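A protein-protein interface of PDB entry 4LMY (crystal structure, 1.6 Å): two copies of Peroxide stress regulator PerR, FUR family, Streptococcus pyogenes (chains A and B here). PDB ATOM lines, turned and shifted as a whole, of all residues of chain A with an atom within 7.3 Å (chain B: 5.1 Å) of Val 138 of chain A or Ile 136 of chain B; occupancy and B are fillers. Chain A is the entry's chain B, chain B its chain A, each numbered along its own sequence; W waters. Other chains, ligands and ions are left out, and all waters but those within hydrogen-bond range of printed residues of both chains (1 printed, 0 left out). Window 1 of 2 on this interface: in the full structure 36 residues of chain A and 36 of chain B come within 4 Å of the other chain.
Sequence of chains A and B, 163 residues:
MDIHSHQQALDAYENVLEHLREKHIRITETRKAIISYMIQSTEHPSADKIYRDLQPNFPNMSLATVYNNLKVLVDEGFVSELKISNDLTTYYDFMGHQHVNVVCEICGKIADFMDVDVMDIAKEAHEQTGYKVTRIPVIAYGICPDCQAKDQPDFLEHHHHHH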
ATOM      1  N   ALA A   9       9.645   7.460   1.107  1.00  0.00           N
ATOM      2  CA  ALA A   9       8.710   6.422   1.520  1.00  0.00           C
ATOM      3  C   ALA A   9       9.435   5.089   1.626  1.00  0.00           C
ATOM      4  O   ALA A   9      10.261   4.754   0.778  1.00  0.00           O
ATOM      5  CB  ALA A   9       7.562   6.323   0.536  1.00  0.00           C
ATOM      6  N   GLN A  98       6.580   2.076   9.303  1.00  0.00           N
ATOM      7  CA  GLN A  98       6.947   2.367   7.926  1.00  0.00           C
ATOM      8  C   GLN A  98       6.817   3.868   7.701  1.00  0.00           C
ATOM      9  O   GLN A  98       6.414   4.608   8.601  1.00  0.00           O
ATOM     10  CB  GLN A  98       6.043   1.613   6.950  1.00  0.00           C
ATOM     11  CG  GLN A  98       4.618   2.118   6.943  1.00  0.00           C
ATOM     12  CD  GLN A  98       3.800   1.555   5.804  1.00  0.00           C
ATOM     13  OE1 GLN A  98       2.578   1.621   5.825  1.00  0.00           O
ATOM     14  NE2 GLN A  98       4.469   1.010   4.796  1.00  0.00           N
ATOM     15  N   HIS A  99       7.143   4.313   6.497  1.00  0.00           N
ATOM     16  CA  HIS A  99       7.021   5.725   6.165  1.00  0.00           C
ATOM     17  C   HIS A  99       6.240   5.902   4.875  1.00  0.00           C
ATOM     18  O   HIS A  99       6.566   5.304   3.852  1.00  0.00           O
ATOM     19  CB  HIS A  99       8.399   6.375   6.076  1.00  0.00           C
ATOM     20  CG  HIS A  99       9.186   6.262   7.342  1.00  0.00           C
ATOM     21  ND1 HIS A  99       9.243   7.273   8.276  1.00  0.00           N
ATOM     22  CD2 HIS A  99       9.917   5.240   7.847  1.00  0.00           C
ATOM     23  CE1 HIS A  99       9.993   6.886   9.294  1.00  0.00           C
ATOM     24  NE2 HIS A  99      10.410   5.655   9.059  1.00  0.00           N
ATOM     25  N   VAL A 100       5.205   6.734   4.946  1.00  0.00           N
ATOM     26  CA  VAL A 100       4.239   6.892   3.868  1.00  0.00           C
ATOM     27  C   VAL A 100       4.249   8.324   3.342  1.00  0.00           C
ATOM     28  O   VAL A 100       4.330   9.275   4.116  1.00  0.00           O
ATOM     29  CB  VAL A 100       2.816   6.551   4.370  1.00  0.00           C
ATOM     30  CG1 VAL A 100       1.777   6.700   3.258  1.00  0.00           C
ATOM     31  CG2 VAL A 100       2.786   5.147   4.961  1.00  0.00           C
ATOM     32  N   ASN A 101       4.166   8.477   2.026  1.00  0.00           N
ATOM     33  CA  ASN A 101       4.098   9.807   1.429  1.00  0.00           C
ATOM     34  C   ASN A 101       2.706  10.422   1.495  1.00  0.00           C
ATOM     35  O   ASN A 101       1.699   9.720   1.404  1.00  0.00           O
ATOM     36  CB  ASN A 101       4.548   9.769  -0.029  1.00  0.00           C
ATOM     37  CG  ASN A 101       6.050   9.686  -0.172  1.00  0.00           C
ATOM     38  OD1 ASN A 101       6.793  10.091   0.721  1.00  0.00           O
ATOM     39  ND2 ASN A 101       6.507   9.175  -1.307  1.00  0.00           N
ATOM     40  N   VAL A 102       2.656  11.737   1.659  1.00  0.00           N
ATOM     41  CA  VAL A 102       1.423  12.474   1.424  1.00  0.00           C
ATOM     42  C   VAL A 102       1.697  13.480   0.310  1.00  0.00           C
ATOM     43  O   VAL A 102       2.647  14.263   0.383  1.00  0.00           O
ATOM     44  CB  VAL A 102       0.864  13.145   2.709  1.00  0.00           C
ATOM     45  CG1 VAL A 102       1.872  14.099   3.327  1.00  0.00           C
ATOM     46  CG2 VAL A 102      -0.445  13.857   2.406  1.00  0.00           C
ATOM     47  N   PHE A 113       5.323  10.739   6.427  1.00  0.00           N
ATOM     48  CA  PHE A 113       5.031  10.581   7.846  1.00  0.00           C
ATOM     49  C   PHE A 113       5.278   9.145   8.299  1.00  0.00           C
ATOM     50  O   PHE A 113       5.346   8.224   7.481  1.00  0.00           O
ATOM     51  CB  PHE A 113       3.593  11.014   8.162  1.00  0.00           C
ATOM     52  CG  PHE A 113       2.539  10.124   7.560  1.00  0.00           C
ATOM     53  CD1 PHE A 113       1.907   9.161   8.328  1.00  0.00           C
ATOM     54  CD2 PHE A 113       2.175  10.258   6.230  1.00  0.00           C
ATOM     55  CE1 PHE A 113       0.934   8.341   7.781  1.00  0.00           C
ATOM     56  CE2 PHE A 113       1.201   9.442   5.675  1.00  0.00           C
ATOM     57  CZ  PHE A 113       0.581   8.486   6.452  1.00  0.00           C
ATOM     58  N   ASP A 115       4.234   5.713   9.959  1.00  0.00           N
ATOM     59  CA  ASP A 115       3.013   4.940  10.126  1.00  0.00           C
ATOM     60  C   ASP A 115       3.237   3.628  10.873  1.00  0.00           C
ATOM     61  O   ASP A 115       4.215   2.926  10.629  1.00  0.00           O
ATOM     62  CB  ASP A 115       2.400   4.640   8.763  1.00  0.00           C
ATOM     63  CG  ASP A 115       1.326   3.582   8.835  1.00  0.00           C
ATOM     64  OD1 ASP A 115       1.575   2.447   8.382  1.00  0.00           O
ATOM     65  OD2 ASP A 115       0.239   3.883   9.363  1.00  0.00           O
ATOM     66  N   VAL A 118      -0.659   0.458   8.971  1.00  0.00           N
ATOM     67  CA  VAL A 118      -0.830  -0.442   7.827  1.00  0.00           C
ATOM     68  C   VAL A 118      -0.580  -1.908   8.187  1.00  0.00           C
ATOM     69  O   VAL A 118      -1.214  -2.804   7.634  1.00  0.00           O
ATOM     70  CB  VAL A 118       0.027  -0.002   6.616  1.00  0.00           C
ATOM     71  CG1 VAL A 118       0.022  -1.057   5.509  1.00  0.00           C
ATOM     72  CG2 VAL A 118      -0.485   1.319   6.077  1.00  0.00           C
ATOM     73  N   ILE A 121      -3.653  -3.260   9.293  1.00  0.00           N
ATOM     74  CA  ILE A 121      -4.483  -3.519   8.123  1.00  0.00           C
ATOM     75  C   ILE A 121      -4.124  -4.882   7.553  1.00  0.00           C
ATOM     76  O   ILE A 121      -4.996  -5.661   7.182  1.00  0.00           O
ATOM     77  CB  ILE A 121      -4.266  -2.453   7.030  1.00  0.00           C
ATOM     78  CG1 ILE A 121      -4.655  -1.071   7.547  1.00  0.00           C
ATOM     79  CG2 ILE A 121      -5.052  -2.788   5.772  1.00  0.00           C
ATOM     80  CD1 ILE A 121      -4.354   0.028   6.573  1.00  0.00           C
ATOM     81  N   ARG A 135       1.839  -7.298   0.248  1.00  0.00           N
ATOM     82  CA  ARG A 135       2.133  -5.871   0.246  1.00  0.00           C
ATOM     83  C   ARG A 135       0.859  -5.035   0.281  1.00  0.00           C
ATOM     84  O   ARG A 135      -0.168  -5.413  -0.283  1.00  0.00           O
ATOM     85  CB  ARG A 135       2.950  -5.504  -0.995  1.00  0.00           C
ATOM     86  CG  ARG A 135       2.215  -5.774  -2.300  1.00  0.00           C
ATOM     87  CD  ARG A 135       3.156  -5.792  -3.494  1.00  0.00           C
ATOM     88  NE  ARG A 135       2.472  -6.238  -4.706  1.00  0.00           N
ATOM     89  CZ  ARG A 135       1.933  -5.425  -5.609  1.00  0.00           C
ATOM     90  NH1 ARG A 135       1.998  -4.109  -5.452  1.00  0.00           N
ATOM     91  NH2 ARG A 135       1.332  -5.930  -6.678  1.00  0.00           N
ATOM     92  N   ILE A 136       0.929  -3.893   0.953  1.00  0.00           N
ATOM     93  CA  ILE A 136      -0.177  -2.949   0.944  1.00  0.00           C
ATOM     94  C   ILE A 136       0.359  -1.557   0.641  1.00  0.00           C
ATOM     95  O   ILE A 136       0.621  -0.777   1.557  1.00  0.00           O
ATOM     96  CB  ILE A 136      -0.938  -2.925   2.286  1.00  0.00           C
ATOM     97  CG1 ILE A 136      -1.332  -4.342   2.715  1.00  0.00           C
ATOM     98  CG2 ILE A 136      -2.169  -2.034   2.183  1.00  0.00           C
ATOM     99  CD1 ILE A 136      -2.161  -4.388   3.979  1.00  0.00           C
ATOM    100  N   PRO A 137       0.545  -1.249  -0.650  1.00  0.00           N
ATOM    101  CA  PRO A 137       1.058   0.071  -1.030  1.00  0.00           C
ATOM    102  C   PRO A 137       0.060   1.160  -0.660  1.00  0.00           C
ATOM    103  O   PRO A 137      -1.119   1.067  -0.996  1.00  0.00           O
ATOM    104  CB  PRO A 137       1.208  -0.034  -2.550  1.00  0.00           C
ATOM    105  CG  PRO A 137       0.257  -1.108  -2.954  1.00  0.00           C
ATOM    106  CD  PRO A 137       0.262  -2.092  -1.825  1.00  0.00           C
ATOM    107  N   VAL A 138       0.531   2.176   0.053  1.00  0.00           N
ATOM    108  CA  VAL A 138      -0.340   3.254   0.490  1.00  0.00           C
ATOM    109  C   VAL A 138       0.299   4.601   0.185  1.00  0.00           C
ATOM    110  O   VAL A 138       1.471   4.820   0.480  1.00  0.00           O
ATOM    111  CB  VAL A 138      -0.634   3.160   2.000  1.00  0.00           C
ATOM    112  CG1 VAL A 138      -1.529   4.301   2.444  1.00  0.00           C
ATOM    113  CG2 VAL A 138      -1.277   1.826   2.335  1.00  0.00           C
ATOM    114  N   ILE A 139      -0.476   5.482  -0.437  1.00  0.00           N
ATOM    115  CA  ILE A 139      -0.078   6.871  -0.636  1.00  0.00           C
ATOM    116  C   ILE A 139      -1.236   7.761  -0.215  1.00  0.00           C
ATOM    117  O   ILE A 139      -2.375   7.538  -0.623  1.00  0.00           O
ATOM    118  CB  ILE A 139       0.259   7.169  -2.105  1.00  0.00           C
ATOM    119  CG1 ILE A 139       1.384   6.256  -2.597  1.00  0.00           C
ATOM    120  CG2 ILE A 139       0.643   8.635  -2.283  1.00  0.00           C
ATOM    121  CD1 ILE A 139       1.786   6.513  -4.030  1.00  0.00           C
ATOM    122  N   ALA A 140      -0.950   8.764   0.608  1.00  0.00           N
ATOM    123  CA  ALA A 140      -1.987   9.695   1.031  1.00  0.00           C
ATOM    124  C   ALA A 140      -1.987  10.927   0.140  1.00  0.00           C
ATOM    125  O   ALA A 140      -0.963  11.290  -0.437  1.00  0.00           O
ATOM    126  CB  ALA A 140      -1.787  10.093   2.483  1.00  0.00           C
ATOM    127  N   TYR A 141      -3.149  11.556   0.015  1.00  0.00           N
ATOM    128  CA  TYR A 141      -3.273  12.790  -0.743  1.00  0.00           C
ATOM    129  C   TYR A 141      -3.898  13.865   0.127  1.00  0.00           C
ATOM    130  O   TYR A 141      -4.666  13.569   1.040  1.00  0.00           O
ATOM    131  CB  TYR A 141      -4.102  12.563  -2.007  1.00  0.00           C
ATOM    132  CG  TYR A 141      -3.445  11.620  -2.982  1.00  0.00           C
ATOM    133  CD1 TYR A 141      -2.602  12.095  -3.978  1.00  0.00           C
ATOM    134  CD2 TYR A 141      -3.660  10.250  -2.903  1.00  0.00           C
ATOM    135  CE1 TYR A 141      -1.992  11.231  -4.870  1.00  0.00           C
ATOM    136  CE2 TYR A 141      -3.054   9.380  -3.789  1.00  0.00           C
ATOM    137  CZ  TYR A 141      -2.223   9.875  -4.771  1.00  0.00           C
ATOM    138  OH  TYR A 141      -1.620   9.009  -5.654  1.00  0.00           O
ATOM    139  N   VAL B 118      -7.420   2.811   8.269  1.00  0.00           N
ATOM    140  CA  VAL B 118      -6.989   3.829   7.303  1.00  0.00           C
ATOM    141  C   VAL B 118      -7.405   5.242   7.723  1.00  0.00           C
ATOM    142  O   VAL B 118      -6.716   6.219   7.419  1.00  0.00           O
ATOM    143  CB  VAL B 118      -7.474   3.511   5.867  1.00  0.00           C
ATOM    144  CG1 VAL B 118      -7.034   4.587   4.882  1.00  0.00           C
ATOM    145  CG2 VAL B 118      -6.935   2.166   5.425  1.00  0.00           C
ATOM    146  N   ILE B 121      -4.708   6.425   9.833  1.00  0.00           N
ATOM    147  CA  ILE B 121      -3.592   6.853   9.000  1.00  0.00           C
ATOM    148  C   ILE B 121      -3.787   8.308   8.596  1.00  0.00           C
ATOM    149  O   ILE B 121      -2.864   9.118   8.680  1.00  0.00           O
ATOM    150  CB  ILE B 121      -3.472   5.989   7.730  1.00  0.00           C
ATOM    151  CG1 ILE B 121      -3.043   4.568   8.088  1.00  0.00           C
ATOM    152  CG2 ILE B 121      -2.485   6.607   6.744  1.00  0.00           C
ATOM    153  CD1 ILE B 121      -3.047   3.626   6.911  1.00  0.00           C
ATOM    154  N   ALA B 122      -5.006   8.630   8.171  1.00  0.00           N
ATOM    155  CA  ALA B 122      -5.355   9.990   7.765  1.00  0.00           C
ATOM    156  C   ALA B 122      -5.104  11.004   8.879  1.00  0.00           C
ATOM    157  O   ALA B 122      -4.600  12.101   8.631  1.00  0.00           O
ATOM    158  CB  ALA B 122      -6.810  10.048   7.309  1.00  0.00           C
ATOM    159  N   ALA B 125      -1.342  11.298   9.321  1.00  0.00           N
ATOM    160  CA  ALA B 125      -0.832  12.019   8.163  1.00  0.00           C
ATOM    161  C   ALA B 125      -1.003  13.524   8.352  1.00  0.00           C
ATOM    162  O   ALA B 125      -0.093  14.304   8.059  1.00  0.00           O
ATOM    163  CB  ALA B 125      -1.530  11.551   6.885  1.00  0.00           C
ATOM    164  N   VAL B 133      -5.793  16.263   4.753  1.00  0.00           N
ATOM    165  CA  VAL B 133      -5.917  15.002   4.027  1.00  0.00           C
ATOM    166  C   VAL B 133      -7.258  14.888   3.305  1.00  0.00           C
ATOM    167  O   VAL B 133      -8.314  15.122   3.892  1.00  0.00           O
ATOM    168  CB  VAL B 133      -5.726  13.798   4.968  1.00  0.00           C
ATOM    169  CG1 VAL B 133      -5.931  12.482   4.215  1.00  0.00           C
ATOM    170  CG2 VAL B 133      -4.348  13.858   5.629  1.00  0.00           C
ATOM    171  N   THR B 134      -7.204  14.530   2.025  1.00  0.00           N
ATOM    172  CA  THR B 134      -8.399  14.450   1.194  1.00  0.00           C
ATOM    173  C   THR B 134      -8.808  13.007   0.910  1.00  0.00           C
ATOM    174  O   THR B 134      -9.997  12.689   0.870  1.00  0.00           O
ATOM    175  CB  THR B 134      -8.198  15.180  -0.149  1.00  0.00           C
ATOM    176  OG1 THR B 134      -7.019  14.681  -0.792  1.00  0.00           O
ATOM    177  CG2 THR B 134      -8.056  16.682   0.070  1.00  0.00           C
ATOM    178  N   ARG B 135      -7.821  12.139   0.708  1.00  0.00           N
ATOM    179  CA  ARG B 135      -8.091  10.744   0.374  1.00  0.00           C
ATOM    180  C   ARG B 135      -6.851   9.886   0.558  1.00  0.00           C
ATOM    181  O   ARG B 135      -5.723  10.359   0.408  1.00  0.00           O
ATOM    182  CB  ARG B 135      -8.574  10.627  -1.072  1.00  0.00           C
ATOM    183  CG  ARG B 135      -7.558  11.107  -2.098  1.00  0.00           C
ATOM    184  CD  ARG B 135      -8.167  11.227  -3.486  1.00  0.00           C
ATOM    185  NE  ARG B 135      -7.247  11.862  -4.426  1.00  0.00           N
ATOM    186  CZ  ARG B 135      -6.469  11.198  -5.275  1.00  0.00           C
ATOM    187  NH1 ARG B 135      -6.504   9.874  -5.314  1.00  0.00           N
ATOM    188  NH2 ARG B 135      -5.660  11.860  -6.090  1.00  0.00           N
ATOM    189  N   ILE B 136      -7.065   8.621   0.902  1.00  0.00           N
ATOM    190  CA  ILE B 136      -5.986   7.647   0.958  1.00  0.00           C
ATOM    191  C   ILE B 136      -6.461   6.340   0.335  1.00  0.00           C
ATOM    192  O   ILE B 136      -6.950   5.455   1.041  1.00  0.00           O
ATOM    193  CB  ILE B 136      -5.525   7.366   2.402  1.00  0.00           C
ATOM    194  CG1 ILE B 136      -5.274   8.666   3.169  1.00  0.00           C
ATOM    195  CG2 ILE B 136      -4.274   6.512   2.398  1.00  0.00           C
ATOM    196  CD1 ILE B 136      -4.757   8.452   4.567  1.00  0.00           C
ATOM    197  N   PRO B 137      -6.340   6.222  -0.995  1.00  0.00           N
ATOM    198  CA  PRO B 137      -6.745   4.981  -1.661  1.00  0.00           C
ATOM    199  C   PRO B 137      -5.855   3.829  -1.212  1.00  0.00           C
ATOM    200  O   PRO B 137      -4.634   3.971  -1.163  1.00  0.00           O
ATOM    201  CB  PRO B 137      -6.531   5.291  -3.146  1.00  0.00           C
ATOM    202  CG  PRO B 137      -5.536   6.399  -3.169  1.00  0.00           C
ATOM    203  CD  PRO B 137      -5.814   7.218  -1.945  1.00  0.00           C
ATOM    204  N   VAL B 138      -6.470   2.706  -0.858  1.00  0.00           N
ATOM    205  CA  VAL B 138      -5.721   1.558  -0.365  1.00  0.00           C
ATOM    206  C   VAL B 138      -6.191   0.271  -1.026  1.00  0.00           C
ATOM    207  O   VAL B 138      -7.387   0.001  -1.099  1.00  0.00           O
ATOM    208  CB  VAL B 138      -5.856   1.409   1.168  1.00  0.00           C
ATOM    209  CG1 VAL B 138      -5.192   0.125   1.640  1.00  0.00           C
ATOM    210  CG2 VAL B 138      -5.255   2.611   1.879  1.00  0.00           C
HETATM  211  O   HOH W   1      -2.820   5.499  -1.912  1.00  0.00           O
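N of Asp 115 of chain A lies within hydrogen-bond range of O of Gln 98 of chain A (2.8 Å). The backbone carbonyl oxygen of Val 100 of chain A is in hydrogen-bond range of the backbone NH of Phe 113 of chain A. The backbone NH (N) of Ala 140 of chain A sits at hydrogen-bond distance from the backbone carbonyl oxygen (O) of Asn 101 of chain A (2.9 Å). OD1 of Asp 115 of chain A sits at hydrogen-bond distance from N of Val 118 of chain A, 3.0 Å away.
N of Thr 134 of chain B lies within hydrogen-bond range of O of Tyr 141 of chain A, 2.9 Å away. O of Arg 135 of chain B lies within hydrogen-bond range of N of Tyr 141 of chain A (2.9 Å).
Val 118 of chain A touches Ile 121 of chain B, and with the chains exchanged Ile 121 of chain A touches Val 118 of chain B. Ile 121 of chain A touches its own counterpart, Ile 121 of chain B. Ile 136 of chain A touches Val 138 of chain B, and with the chains exchanged Val 138 of chain A touches Ile 136 of chain B.
Ile 136 of chain B touches three residues of chain A. Printed residues of chain A within 4 Å of Thr 134 of chain B: Tyr 141. Of the printed residues of chain B, Ala 140 of chain A touches Arg 135 (3.8 Å) and Ile 136 (3.8 Å). Of the printed residues of chain A, Val 133 of chain B touches Tyr 141 (3.5 Å). Of the printed residues of chain A, Arg 135 of chain B touches Ala 140 (3.8 Å) and Tyr 141 (2.9 Å). Val 100 of chain A touches none of the printed residues of chain B. The nearest residue of chain B that does not touch Val 138 of chain A is Val 138 of chain B (4.1 Å). The nearest residue of chain A that does not touch Ile 136 of chain B is Tyr 141 of chain A (4.8 Å).
Water W1 lies within hydrogen-bond range of O of Ile 139 of chain A (2.5 Å) and O of Pro 137 of chain B (2.5 Å).
Among the printed residues, pairs that only touch across the chains: Val 138 of chain A with Ile 136 of chain B (3.5 Å), Tyr 141 of chain A with Val 133 of chain B (3.5 Å), Ile 121 of chain A with Val 118 of chain B (3.5 Å), Val 118 of chain A with Ile 121 of chain B (3.5 Å), Asp 115 of chain A with Ile 121 of chain B (3.6 Å), Phe 113 of chain A with Ile 121 of chain B (3.6 Å), Phe 113 of chain A with Ala 125 of chain B (3.7 Å), Ile 139 of chain A with Pro 137 of chain B (3.7 Å), Ile 139 of chain A with Ile 136 of chain B (3.7 Å), Ile 136 of chain A with Val 138 of chain B (3.8 Å), Ala 140 of chain A with Arg 135 of chain B (3.8 Å), Ala 140 of chain A with Ile 136 of chain B (3.8 Å), Tyr 141 of chain A with Pro 137 of chain B (3.8 Å) and Ile 121 of chain A with Ile 121 of chain B (3.8 Å).
Printed residues of chain B that touch a printed residue of chain A: Val 118, Ile 121, Ala 125, Val 133, Thr 134, Arg 135, Ile 136, Pro 137 and Val 138. Hydrophobic or aromatic side chains of chain B that line the printed part of chain A: Val 118, Ile 121, Ala 125, Val 133, Ile 136, Pro 137 and Val 138. Printed residues of chain A that touch a printed residue of chain B: Phe 113, Asp 115, Val 118, Ile 121, Ile 136, Val 138, Ile 139, Ala 140 and Tyr 141. Hydrophobic or aromatic side chains of chain A within 4 Å of the printed part of chain B: Phe 113, Val 118, Ile 121, Ile 136, Val 138, Ala 140 and Tyr 141. Among the printed residues, no Asp or Glu carboxylate lies within 4 Å of a Lys or Arg side-chain nitrogen of the other chain.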
